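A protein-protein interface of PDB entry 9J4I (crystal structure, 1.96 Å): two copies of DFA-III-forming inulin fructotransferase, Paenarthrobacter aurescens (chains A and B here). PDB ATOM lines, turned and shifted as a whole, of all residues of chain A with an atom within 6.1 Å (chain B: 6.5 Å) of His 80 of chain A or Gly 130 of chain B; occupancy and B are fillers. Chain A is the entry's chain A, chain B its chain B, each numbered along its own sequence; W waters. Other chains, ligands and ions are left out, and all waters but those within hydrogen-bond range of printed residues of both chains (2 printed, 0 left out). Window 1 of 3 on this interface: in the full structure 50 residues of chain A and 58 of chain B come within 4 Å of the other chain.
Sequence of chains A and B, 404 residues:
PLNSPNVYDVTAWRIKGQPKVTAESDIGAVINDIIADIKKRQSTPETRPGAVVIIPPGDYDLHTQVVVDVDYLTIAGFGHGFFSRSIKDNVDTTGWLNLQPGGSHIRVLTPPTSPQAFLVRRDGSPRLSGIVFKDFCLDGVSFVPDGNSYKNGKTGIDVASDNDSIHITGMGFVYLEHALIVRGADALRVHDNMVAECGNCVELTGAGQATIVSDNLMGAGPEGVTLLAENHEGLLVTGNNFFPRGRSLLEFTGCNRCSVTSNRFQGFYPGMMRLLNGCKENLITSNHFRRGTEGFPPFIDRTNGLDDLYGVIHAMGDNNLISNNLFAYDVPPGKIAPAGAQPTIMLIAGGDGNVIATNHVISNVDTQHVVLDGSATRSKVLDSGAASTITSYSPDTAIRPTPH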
ATOM      1  N   PHE A  78      13.388  22.834  -7.216  1.00  0.00           N
ATOM      2  CA  PHE A  78      13.360  22.771  -8.699  1.00  0.00           C
ATOM      3  C   PHE A  78      12.313  23.727  -9.279  1.00  0.00           C
ATOM      4  O   PHE A  78      12.070  23.688 -10.519  1.00  0.00           O
ATOM      5  CB  PHE A  78      13.112  21.328  -9.131  1.00  0.00           C
ATOM      6  CG  PHE A  78      14.219  20.366  -8.784  1.00  0.00           C
ATOM      7  CD1 PHE A  78      15.290  20.194  -9.632  1.00  0.00           C
ATOM      8  CD2 PHE A  78      14.188  19.622  -7.613  1.00  0.00           C
ATOM      9  CE1 PHE A  78      16.293  19.284  -9.339  1.00  0.00           C
ATOM     10  CE2 PHE A  78      15.197  18.719  -7.318  1.00  0.00           C
ATOM     11  CZ  PHE A  78      16.247  18.546  -8.188  1.00  0.00           C
ATOM     12  N   GLY A  79      11.717  24.576  -8.445  1.00  0.00           N
ATOM     13  CA  GLY A  79      10.640  25.464  -8.907  1.00  0.00           C
ATOM     14  C   GLY A  79      10.107  26.365  -7.810  1.00  0.00           C
ATOM     15  O   GLY A  79       9.838  25.880  -6.686  1.00  0.00           O
ATOM     16  N   HIS A  80       9.888  27.626  -8.171  1.00  0.00           N
ATOM     17  CA  HIS A  80       9.340  28.700  -7.313  1.00  0.00           C
ATOM     18  C   HIS A  80       7.840  28.482  -7.007  1.00  0.00           C
ATOM     19  O   HIS A  80       7.383  29.066  -6.014  1.00  0.00           O
ATOM     20  CB  HIS A  80       9.647  30.046  -7.977  1.00  0.00           C
ATOM     21  CG  HIS A  80       8.930  30.273  -9.263  1.00  0.00           C
ATOM     22  ND1 HIS A  80       9.252  29.599 -10.419  1.00  0.00           N
ATOM     23  CD2 HIS A  80       7.936  31.126  -9.590  1.00  0.00           C
ATOM     24  CE1 HIS A  80       8.477  30.019 -11.397  1.00  0.00           C
ATOM     25  NE2 HIS A  80       7.661  30.963 -10.917  1.00  0.00           N
ATOM     26  N   GLY A  81       7.106  27.741  -7.847  1.00  0.00           N
ATOM     27  CA  GLY A  81       5.722  27.262  -7.605  1.00  0.00           C
ATOM     28  C   GLY A  81       4.685  28.355  -7.354  1.00  0.00           C
ATOM     29  O   GLY A  81       3.630  28.043  -6.742  1.00  0.00           O
ATOM     30  N   PHE A  82       4.909  29.588  -7.813  1.00  0.00           N
ATOM     31  CA  PHE A  82       4.025  30.730  -7.464  1.00  0.00           C
ATOM     32  C   PHE A  82       2.616  30.533  -8.064  1.00  0.00           C
ATOM     33  O   PHE A  82       2.478  30.110  -9.223  1.00  0.00           O
ATOM     34  CB  PHE A  82       4.599  32.076  -7.883  1.00  0.00           C
ATOM     35  CG  PHE A  82       3.686  33.194  -7.458  1.00  0.00           C
ATOM     36  CD1 PHE A  82       3.804  33.761  -6.205  1.00  0.00           C
ATOM     37  CD2 PHE A  82       2.649  33.608  -8.276  1.00  0.00           C
ATOM     38  CE1 PHE A  82       2.919  34.746  -5.787  1.00  0.00           C
ATOM     39  CE2 PHE A  82       1.778  34.607  -7.866  1.00  0.00           C
ATOM     40  CZ  PHE A  82       1.920  35.179  -6.626  1.00  0.00           C
ATOM     41  N   PRO A 101      -0.304  27.031  -4.510  1.00  0.00           N
ATOM     42  CA  PRO A 101       1.049  27.032  -5.069  1.00  0.00           C
ATOM     43  C   PRO A 101       1.654  25.627  -5.097  1.00  0.00           C
ATOM     44  O   PRO A 101       1.127  24.708  -4.470  1.00  0.00           O
ATOM     45  CB  PRO A 101       1.842  27.951  -4.135  1.00  0.00           C
ATOM     46  CG  PRO A 101       0.794  28.778  -3.406  1.00  0.00           C
ATOM     47  CD  PRO A 101      -0.418  27.884  -3.315  1.00  0.00           C
ATOM     48  N   GLY A 102       2.747  25.475  -5.839  1.00  0.00           N
ATOM     49  CA  GLY A 102       3.371  24.158  -6.048  1.00  0.00           C
ATOM     50  C   GLY A 102       4.871  24.278  -6.169  1.00  0.00           C
ATOM     51  O   GLY A 102       5.456  25.069  -5.413  1.00  0.00           O
ATOM     52  N   GLY A 103       5.446  23.529  -7.098  1.00  0.00           N
ATOM     53  CA  GLY A 103       6.897  23.428  -7.289  1.00  0.00           C
ATOM     54  C   GLY A 103       7.490  22.716  -6.096  1.00  0.00           C
ATOM     55  O   GLY A 103       6.851  21.764  -5.615  1.00  0.00           O
ATOM     56  N   SER A 104       8.614  23.209  -5.569  1.00  0.00           N
ATOM     57  CA  SER A 104       9.226  22.697  -4.309  1.00  0.00           C
ATOM     58  C   SER A 104       8.554  23.443  -3.148  1.00  0.00           C
ATOM     59  O   SER A 104       9.099  24.457  -2.666  1.00  0.00           O
ATOM     60  CB  SER A 104      10.724  22.813  -4.342  1.00  0.00           C
ATOM     61  OG  SER A 104      11.262  22.001  -5.390  1.00  0.00           O
ATOM     62  N   ASP A 135      15.241  28.447  -5.684  1.00  0.00           N
ATOM     63  CA  ASP A 135      14.386  27.585  -6.543  1.00  0.00           C
ATOM     64  C   ASP A 135      13.395  26.792  -5.688  1.00  0.00           C
ATOM     65  O   ASP A 135      13.061  25.648  -6.071  1.00  0.00           O
ATOM     66  CB  ASP A 135      15.257  26.631  -7.376  1.00  0.00           C
ATOM     67  CG  ASP A 135      16.261  27.319  -8.287  1.00  0.00           C
ATOM     68  OD1 ASP A 135      15.960  28.446  -8.743  1.00  0.00           O
ATOM     69  OD2 ASP A 135      17.346  26.718  -8.530  1.00  0.00           O
ATOM     70  N   PHE A 136      12.877  27.350  -4.598  1.00  0.00           N
ATOM     71  CA  PHE A 136      11.722  26.724  -3.918  1.00  0.00           C
ATOM     72  C   PHE A 136      10.706  27.781  -3.486  1.00  0.00           C
ATOM     73  O   PHE A 136      10.880  29.015  -3.675  1.00  0.00           O
ATOM     74  CB  PHE A 136      12.139  25.778  -2.790  1.00  0.00           C
ATOM     75  CG  PHE A 136      12.710  26.398  -1.544  1.00  0.00           C
ATOM     76  CD1 PHE A 136      14.071  26.650  -1.443  1.00  0.00           C
ATOM     77  CD2 PHE A 136      11.909  26.603  -0.429  1.00  0.00           C
ATOM     78  CE1 PHE A 136      14.605  27.182  -0.279  1.00  0.00           C
ATOM     79  CE2 PHE A 136      12.453  27.124   0.737  1.00  0.00           C
ATOM     80  CZ  PHE A 136      13.801  27.390   0.817  1.00  0.00           C
ATOM     81  N   CYS A 137       9.592  27.270  -2.987  1.00  0.00           N
ATOM     82  CA  CYS A 137       8.383  28.071  -2.699  1.00  0.00           C
ATOM     83  C   CYS A 137       8.138  28.104  -1.196  1.00  0.00           C
ATOM     84  O   CYS A 137       8.140  27.033  -0.570  1.00  0.00           O
ATOM     85  CB  CYS A 137       7.189  27.466  -3.417  1.00  0.00           C
ATOM     86  SG  CYS A 137       5.675  28.388  -3.068  1.00  0.00           S
ATOM     87  N   LEU A 138       7.976  29.299  -0.634  1.00  0.00           N
ATOM     88  CA  LEU A 138       7.559  29.480   0.773  1.00  0.00           C
ATOM     89  C   LEU A 138       6.164  30.107   0.734  1.00  0.00           C
ATOM     90  O   LEU A 138       6.005  31.241   0.222  1.00  0.00           O
ATOM     91  CB  LEU A 138       8.595  30.305   1.546  1.00  0.00           C
ATOM     92  CG  LEU A 138       9.842  29.520   1.954  1.00  0.00           C
ATOM     93  CD1 LEU A 138      10.998  30.446   2.297  1.00  0.00           C
ATOM     94  CD2 LEU A 138       9.534  28.571   3.106  1.00  0.00           C
ATOM     95  N   GLY A 170      15.745  32.690  -7.548  1.00  0.00           N
ATOM     96  CA  GLY A 170      14.795  31.732  -8.147  1.00  0.00           C
ATOM     97  C   GLY A 170      13.725  31.277  -7.172  1.00  0.00           C
ATOM     98  O   GLY A 170      13.086  30.232  -7.449  1.00  0.00           O
ATOM     99  N   MET A 171      13.507  32.037  -6.099  1.00  0.00           N
ATOM    100  CA  MET A 171      12.551  31.675  -5.017  1.00  0.00           C
ATOM    101  C   MET A 171      11.151  32.139  -5.431  1.00  0.00           C
ATOM    102  O   MET A 171      11.033  33.031  -6.286  1.00  0.00           O
ATOM    103  CB  MET A 171      12.907  32.331  -3.673  1.00  0.00           C
ATOM    104  CG  MET A 171      14.194  31.813  -3.025  1.00  0.00           C
ATOM    105  SD  MET A 171      14.138  30.111  -2.510  1.00  0.00           S
ATOM    106  CE  MET A 171      12.875  30.200  -1.236  1.00  0.00           C
ATOM    107  N   GLY A 172      10.141  31.526  -4.820  1.00  0.00           N
ATOM    108  CA  GLY A 172       8.757  32.022  -4.789  1.00  0.00           C
ATOM    109  C   GLY A 172       8.346  32.203  -3.350  1.00  0.00           C
ATOM    110  O   GLY A 172       8.604  31.298  -2.534  1.00  0.00           O
ATOM    111  N   PHE A 173       7.818  33.377  -3.025  1.00  0.00           N
ATOM    112  CA  PHE A 173       7.229  33.691  -1.707  1.00  0.00           C
ATOM    113  C   PHE A 173       5.793  34.140  -1.963  1.00  0.00           C
ATOM    114  O   PHE A 173       5.567  34.982  -2.864  1.00  0.00           O
ATOM    115  CB  PHE A 173       7.995  34.790  -0.984  1.00  0.00           C
ATOM    116  CG  PHE A 173       9.457  34.545  -0.739  1.00  0.00           C
ATOM    117  CD1 PHE A 173      10.398  34.850  -1.714  1.00  0.00           C
ATOM    118  CD2 PHE A 173       9.902  34.092   0.499  1.00  0.00           C
ATOM    119  CE1 PHE A 173      11.754  34.702  -1.462  1.00  0.00           C
ATOM    120  CE2 PHE A 173      11.265  33.955   0.746  1.00  0.00           C
ATOM    121  CZ  PHE A 173      12.184  34.242  -0.243  1.00  0.00           C
ATOM    122  N   MET A 194      10.451  35.682  -7.216  1.00  0.00           N
ATOM    123  CA  MET A 194       9.018  36.054  -7.290  1.00  0.00           C
ATOM    124  C   MET A 194       8.563  36.236  -5.845  1.00  0.00           C
ATOM    125  O   MET A 194       8.531  35.232  -5.118  1.00  0.00           O
ATOM    126  CB  MET A 194       8.218  34.948  -7.975  1.00  0.00           C
ATOM    127  CG  MET A 194       6.713  35.200  -8.021  1.00  0.00           C
ATOM    128  SD  MET A 194       6.302  36.304  -9.392  1.00  0.00           S
ATOM    129  CE  MET A 194       4.539  36.559  -9.161  1.00  0.00           C
ATOM    130  N   ASP B  71       0.585  22.905 -14.092  1.00  0.00           N
ATOM    131  CA  ASP B  71       1.269  23.995 -13.360  1.00  0.00           C
ATOM    132  C   ASP B  71       2.574  23.463 -12.769  1.00  0.00           C
ATOM    133  O   ASP B  71       2.644  22.284 -12.432  1.00  0.00           O
ATOM    134  CB  ASP B  71       0.386  24.576 -12.261  1.00  0.00           C
ATOM    135  CG  ASP B  71      -1.012  24.927 -12.734  1.00  0.00           C
ATOM    136  OD1 ASP B  71      -1.174  26.011 -13.344  1.00  0.00           O
ATOM    137  OD2 ASP B  71      -1.916  24.098 -12.502  1.00  0.00           O
ATOM    138  N   TYR B  72       3.590  24.318 -12.660  1.00  0.00           N
ATOM    139  CA  TYR B  72       4.809  24.020 -11.865  1.00  0.00           C
ATOM    140  C   TYR B  72       5.514  22.811 -12.476  1.00  0.00           C
ATOM    141  O   TYR B  72       6.174  22.036 -11.775  1.00  0.00           O
ATOM    142  CB  TYR B  72       4.468  23.768 -10.394  1.00  0.00           C
ATOM    143  CG  TYR B  72       3.266  24.507  -9.860  1.00  0.00           C
ATOM    144  CD1 TYR B  72       3.203  25.893  -9.882  1.00  0.00           C
ATOM    145  CD2 TYR B  72       2.207  23.816  -9.294  1.00  0.00           C
ATOM    146  CE1 TYR B  72       2.084  26.572  -9.433  1.00  0.00           C
ATOM    147  CE2 TYR B  72       1.094  24.482  -8.806  1.00  0.00           C
ATOM    148  CZ  TYR B  72       1.033  25.862  -8.880  1.00  0.00           C
ATOM    149  OH  TYR B  72      -0.058  26.521  -8.415  1.00  0.00           O
ATOM    150  N   LEU B  73       5.429  22.662 -13.792  1.00  0.00           N
ATOM    151  CA  LEU B  73       6.354  21.754 -14.493  1.00  0.00           C
ATOM    152  C   LEU B  73       7.677  22.503 -14.701  1.00  0.00           C
ATOM    153  O   LEU B  73       7.648  23.597 -15.286  1.00  0.00           O
ATOM    154  CB  LEU B  73       5.754  21.296 -15.823  1.00  0.00           C
ATOM    155  CG  LEU B  73       6.590  20.239 -16.539  1.00  0.00           C
ATOM    156  CD1 LEU B  73       6.749  19.009 -15.660  1.00  0.00           C
ATOM    157  CD2 LEU B  73       5.981  19.866 -17.888  1.00  0.00           C
ATOM    158  N   THR B  74       8.791  21.915 -14.253  1.00  0.00           N
ATOM    159  CA  THR B  74      10.165  22.357 -14.587  1.00  0.00           C
ATOM    160  C   THR B  74      10.735  21.378 -15.617  1.00  0.00           C
ATOM    161  O   THR B  74      10.756  20.179 -15.333  1.00  0.00           O
ATOM    162  CB  THR B  74      11.027  22.452 -13.324  1.00  0.00           C
ATOM    163  OG1 THR B  74      10.430  23.400 -12.438  1.00  0.00           O
ATOM    164  CG2 THR B  74      12.449  22.849 -13.632  1.00  0.00           C
ATOM    165  N   LEU B 128      -2.264  28.842 -16.367  1.00  0.00           N
ATOM    166  CA  LEU B 128      -1.076  27.986 -16.136  1.00  0.00           C
ATOM    167  C   LEU B 128      -0.047  28.822 -15.363  1.00  0.00           C
ATOM    168  O   LEU B 128       0.186  29.986 -15.746  1.00  0.00           O
ATOM    169  CB  LEU B 128      -0.533  27.485 -17.471  1.00  0.00           C
ATOM    170  CG  LEU B 128      -1.240  26.266 -18.060  1.00  0.00           C
ATOM    171  CD1 LEU B 128      -0.707  25.983 -19.451  1.00  0.00           C
ATOM    172  CD2 LEU B 128      -1.080  25.039 -17.170  1.00  0.00           C
ATOM    173  N   SER B 129       0.472  28.283 -14.262  1.00  0.00           N
ATOM    174  CA  SER B 129       1.285  29.031 -13.276  1.00  0.00           C
ATOM    175  C   SER B 129       2.626  28.331 -13.047  1.00  0.00           C
ATOM    176  O   SER B 129       2.636  27.105 -12.935  1.00  0.00           O
ATOM    177  CB  SER B 129       0.545  29.214 -11.969  1.00  0.00           C
ATOM    178  OG  SER B 129      -0.660  29.934 -12.165  1.00  0.00           O
ATOM    179  N   GLY B 130       3.700  29.125 -12.931  1.00  0.00           N
ATOM    180  CA  GLY B 130       4.976  28.700 -12.338  1.00  0.00           C
ATOM    181  C   GLY B 130       5.657  27.610 -13.136  1.00  0.00           C
ATOM    182  O   GLY B 130       6.467  26.903 -12.547  1.00  0.00           O
ATOM    183  N   ILE B 131       5.410  27.534 -14.449  1.00  0.00           N
ATOM    184  CA  ILE B 131       6.181  26.644 -15.357  1.00  0.00           C
ATOM    185  C   ILE B 131       7.585  27.238 -15.563  1.00  0.00           C
ATOM    186  O   ILE B 131       7.716  28.475 -15.728  1.00  0.00           O
ATOM    187  CB  ILE B 131       5.415  26.399 -16.665  1.00  0.00           C
ATOM    188  CG1 ILE B 131       4.117  25.637 -16.370  1.00  0.00           C
ATOM    189  CG2 ILE B 131       6.285  25.666 -17.666  1.00  0.00           C
ATOM    190  CD1 ILE B 131       3.125  25.697 -17.479  1.00  0.00           C
ATOM    191  N   VAL B 132       8.597  26.376 -15.508  1.00  0.00           N
ATOM    192  CA  VAL B 132      10.034  26.745 -15.629  1.00  0.00           C
ATOM    193  C   VAL B 132      10.632  25.942 -16.785  1.00  0.00           C
ATOM    194  O   VAL B 132      10.600  24.707 -16.724  1.00  0.00           O
ATOM    195  CB  VAL B 132      10.817  26.503 -14.319  1.00  0.00           C
ATOM    196  CG1 VAL B 132      12.279  26.923 -14.452  1.00  0.00           C
ATOM    197  CG2 VAL B 132      10.171  27.194 -13.129  1.00  0.00           C
ATOM    198  N   ASP B 164       0.843  32.705 -15.711  1.00  0.00           N
ATOM    199  CA  ASP B 164       1.314  33.527 -14.568  1.00  0.00           C
ATOM    200  C   ASP B 164       2.639  32.965 -14.036  1.00  0.00           C
ATOM    201  O   ASP B 164       2.727  31.752 -13.809  1.00  0.00           O
ATOM    202  CB  ASP B 164       0.268  33.547 -13.459  1.00  0.00           C
ATOM    203  CG  ASP B 164       0.529  34.573 -12.374  1.00  0.00           C
ATOM    204  OD1 ASP B 164       1.094  35.626 -12.702  1.00  0.00           O
ATOM    205  OD2 ASP B 164       0.118  34.321 -11.217  1.00  0.00           O
ATOM    206  N   SER B 165       3.629  33.832 -13.832  1.00  0.00           N
ATOM    207  CA  SER B 165       4.887  33.489 -13.118  1.00  0.00           C
ATOM    208  C   SER B 165       5.638  32.386 -13.858  1.00  0.00           C
ATOM    209  O   SER B 165       6.219  31.524 -13.184  1.00  0.00           O
ATOM    210  CB  SER B 165       4.604  33.083 -11.689  1.00  0.00           C
ATOM    211  OG  SER B 165       5.779  33.210 -10.890  1.00  0.00           O
ATOM    212  N   ILE B 166       5.655  32.420 -15.198  1.00  0.00           N
ATOM    213  CA  ILE B 166       6.524  31.511 -15.994  1.00  0.00           C
ATOM    214  C   ILE B 166       7.961  32.056 -15.927  1.00  0.00           C
ATOM    215  O   ILE B 166       8.137  33.294 -15.837  1.00  0.00           O
ATOM    216  CB  ILE B 166       5.995  31.341 -17.432  1.00  0.00           C
ATOM    217  CG1 ILE B 166       4.668  30.568 -17.421  1.00  0.00           C
ATOM    218  CG2 ILE B 166       7.034  30.663 -18.319  1.00  0.00           C
ATOM    219  CD1 ILE B 166       4.189  30.119 -18.780  1.00  0.00           C
ATOM    220  N   HIS B 167       8.944  31.166 -15.940  1.00  0.00           N
ATOM    221  CA  HIS B 167      10.385  31.511 -15.814  1.00  0.00           C
ATOM    222  C   HIS B 167      11.150  30.726 -16.876  1.00  0.00           C
ATOM    223  O   HIS B 167      11.128  29.462 -16.822  1.00  0.00           O
ATOM    224  CB  HIS B 167      10.880  31.243 -14.395  1.00  0.00           C
ATOM    225  CG  HIS B 167      12.184  31.874 -14.010  1.00  0.00           C
ATOM    226  ND1 HIS B 167      12.882  31.448 -12.894  1.00  0.00           N
ATOM    227  CD2 HIS B 167      12.921  32.873 -14.554  1.00  0.00           C
ATOM    228  CE1 HIS B 167      13.976  32.184 -12.737  1.00  0.00           C
ATOM    229  NE2 HIS B 167      14.021  33.074 -13.746  1.00  0.00           N
ATOM    230  N   ALA B 187       3.589  38.434 -15.212  1.00  0.00           N
ATOM    231  CA  ALA B 187       4.677  38.173 -14.240  1.00  0.00           C
ATOM    232  C   ALA B 187       5.632  37.120 -14.827  1.00  0.00           C
ATOM    233  O   ALA B 187       6.161  36.288 -14.071  1.00  0.00           O
ATOM    234  CB  ALA B 187       4.066  37.746 -12.927  1.00  0.00           C
ATOM    235  N   ARG B 189       9.217  36.064 -16.549  1.00  0.00           N
ATOM    236  CA  ARG B 189      10.658  36.421 -16.613  1.00  0.00           C
ATOM    237  C   ARG B 189      11.330  35.594 -17.724  1.00  0.00           C
ATOM    238  O   ARG B 189      11.306  34.350 -17.683  1.00  0.00           O
ATOM    239  CB  ARG B 189      11.336  36.220 -15.254  1.00  0.00           C
ATOM    240  CG  ARG B 189      10.934  37.217 -14.175  1.00  0.00           C
ATOM    241  CD  ARG B 189      11.359  36.709 -12.804  1.00  0.00           C
ATOM    242  NE  ARG B 189      10.563  35.557 -12.393  1.00  0.00           N
ATOM    243  CZ  ARG B 189      10.923  34.645 -11.493  1.00  0.00           C
ATOM    244  NH1 ARG B 189      12.104  34.703 -10.892  1.00  0.00           N
ATOM    245  NH2 ARG B 189      10.093  33.668 -11.190  1.00  0.00           N
HETATM  246  O   HOH W   1      11.510  32.537  -9.085  1.00  0.00           O
HETATM  247  O   HOH W   2       7.478  25.919 -10.171  1.00  0.00           O
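Printed residues of chain B within 4 Å of His 80 of chain A: Gly 130, Val 132, Ser 165 and Arg 189. Gly 130 of chain B touches just one residue of chain A: His 80. Printed residues of chain A within 4 Å of Arg 189 of chain B: His 80 (3.6 Å) and Met 194 (3.9 Å). Of the printed residues of chain B, Gly 103 of chain A touches Tyr 72. The nearest residue of chain B that does not touch His 80 of chain A is His 167 of chain B (4.03 Å).
No position is printed for both chains.
Among the printed residues, pairs that only touch across the chains: His 80 of chain A with Gly 130 of chain B (3.8 Å), His 80 of chain A with Val 132 of chain B (3.7 Å), His 80 of chain A with Arg 189 of chain B (3.6 Å), Gly 81 of chain A with Tyr 72 of chain B (3.4 Å), Phe 82 of chain A with Tyr 72 of chain B (3.6 Å), Phe 82 of chain A with Ser 129 of chain B (3.5 Å), Phe 82 of chain A with Asp 164 of chain B (3.8 Å), Phe 82 of chain A with Ser 165 of chain B (3.4 Å), Pro 101 of chain A with Tyr 72 of chain B (3.6 Å), Gly 102 of chain A with Tyr 72 of chain B (3.5 Å), Gly 103 of chain A with Tyr 72 of chain B (3.4 Å), Met 194 of chain A with Ala 187 of chain B (3.98 Å) and Met 194 of chain A with Arg 189 of chain B (3.9 Å).
The backbone NH (N) of Phe 78 of chain A lies within hydrogen-bond range of the side-chain hydroxyl (OG) of Ser 104 of chain A, 2.9 Å away. O of Gly 81 of chain A lies within hydrogen-bond range of N of Gly 102 of chain A (2.9 Å). The backbone NH of Met 194 of chain A is in hydrogen-bond range of the backbone carbonyl oxygen of Met 171 of chain A. The side-chain carboxylate (OD1) of Asp 71 of chain B lies within hydrogen-bond range of the backbone NH (N) of Ser 129 of chain B, at 3.0 Å. N of Tyr 72 of chain B sits at hydrogen-bond distance from O of Ser 129 of chain B (3.0 Å). O of Leu 128 of chain B lies within hydrogen-bond range of N of Asp 164 of chain B (2.8 Å).
The side-chain hydroxyl of Thr 74 of chain B is in hydrogen-bond range of the backbone carbonyl oxygen of Phe 78 of chain A. A ring nitrogen (NE2) of His 80 of chain A lies within hydrogen-bond range of the backbone carbonyl oxygen of Ser 165 of chain B (2.7 Å). The side-chain sulfur (SD) of Met 194 of chain A sits at hydrogen-bond distance from the side-chain hydroxyl (OG) of Ser 165 of chain B, 3.5 Å away.
Of the 18 printed residues of chain A, 8 touch a printed residue of chain B. Printed residues of chain B that touch a printed residue of chain A: Tyr 72, Thr 74, Ser 129, Gly 130, Val 132, Asp 164, Ser 165, Ala 187 and Arg 189. Hydrophobic or aromatic side chains of chain B that line the printed part of chain A: Tyr 72, Val 132 and Ala 187. Among the printed residues, 16 pairs touch across the chains.
Water W2 lies within hydrogen-bond range of O of Gly 130 of chain B (2.8 Å) and N of Gly 81 of chain A (3.0 Å). Water W1 lies within hydrogen-bond range of the guanidinium group of Arg 189 of chain B, the backbone carbonyl oxygen of Met 171 of chain A and the backbone carbonyl oxygen of Gly 170 of chain A.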
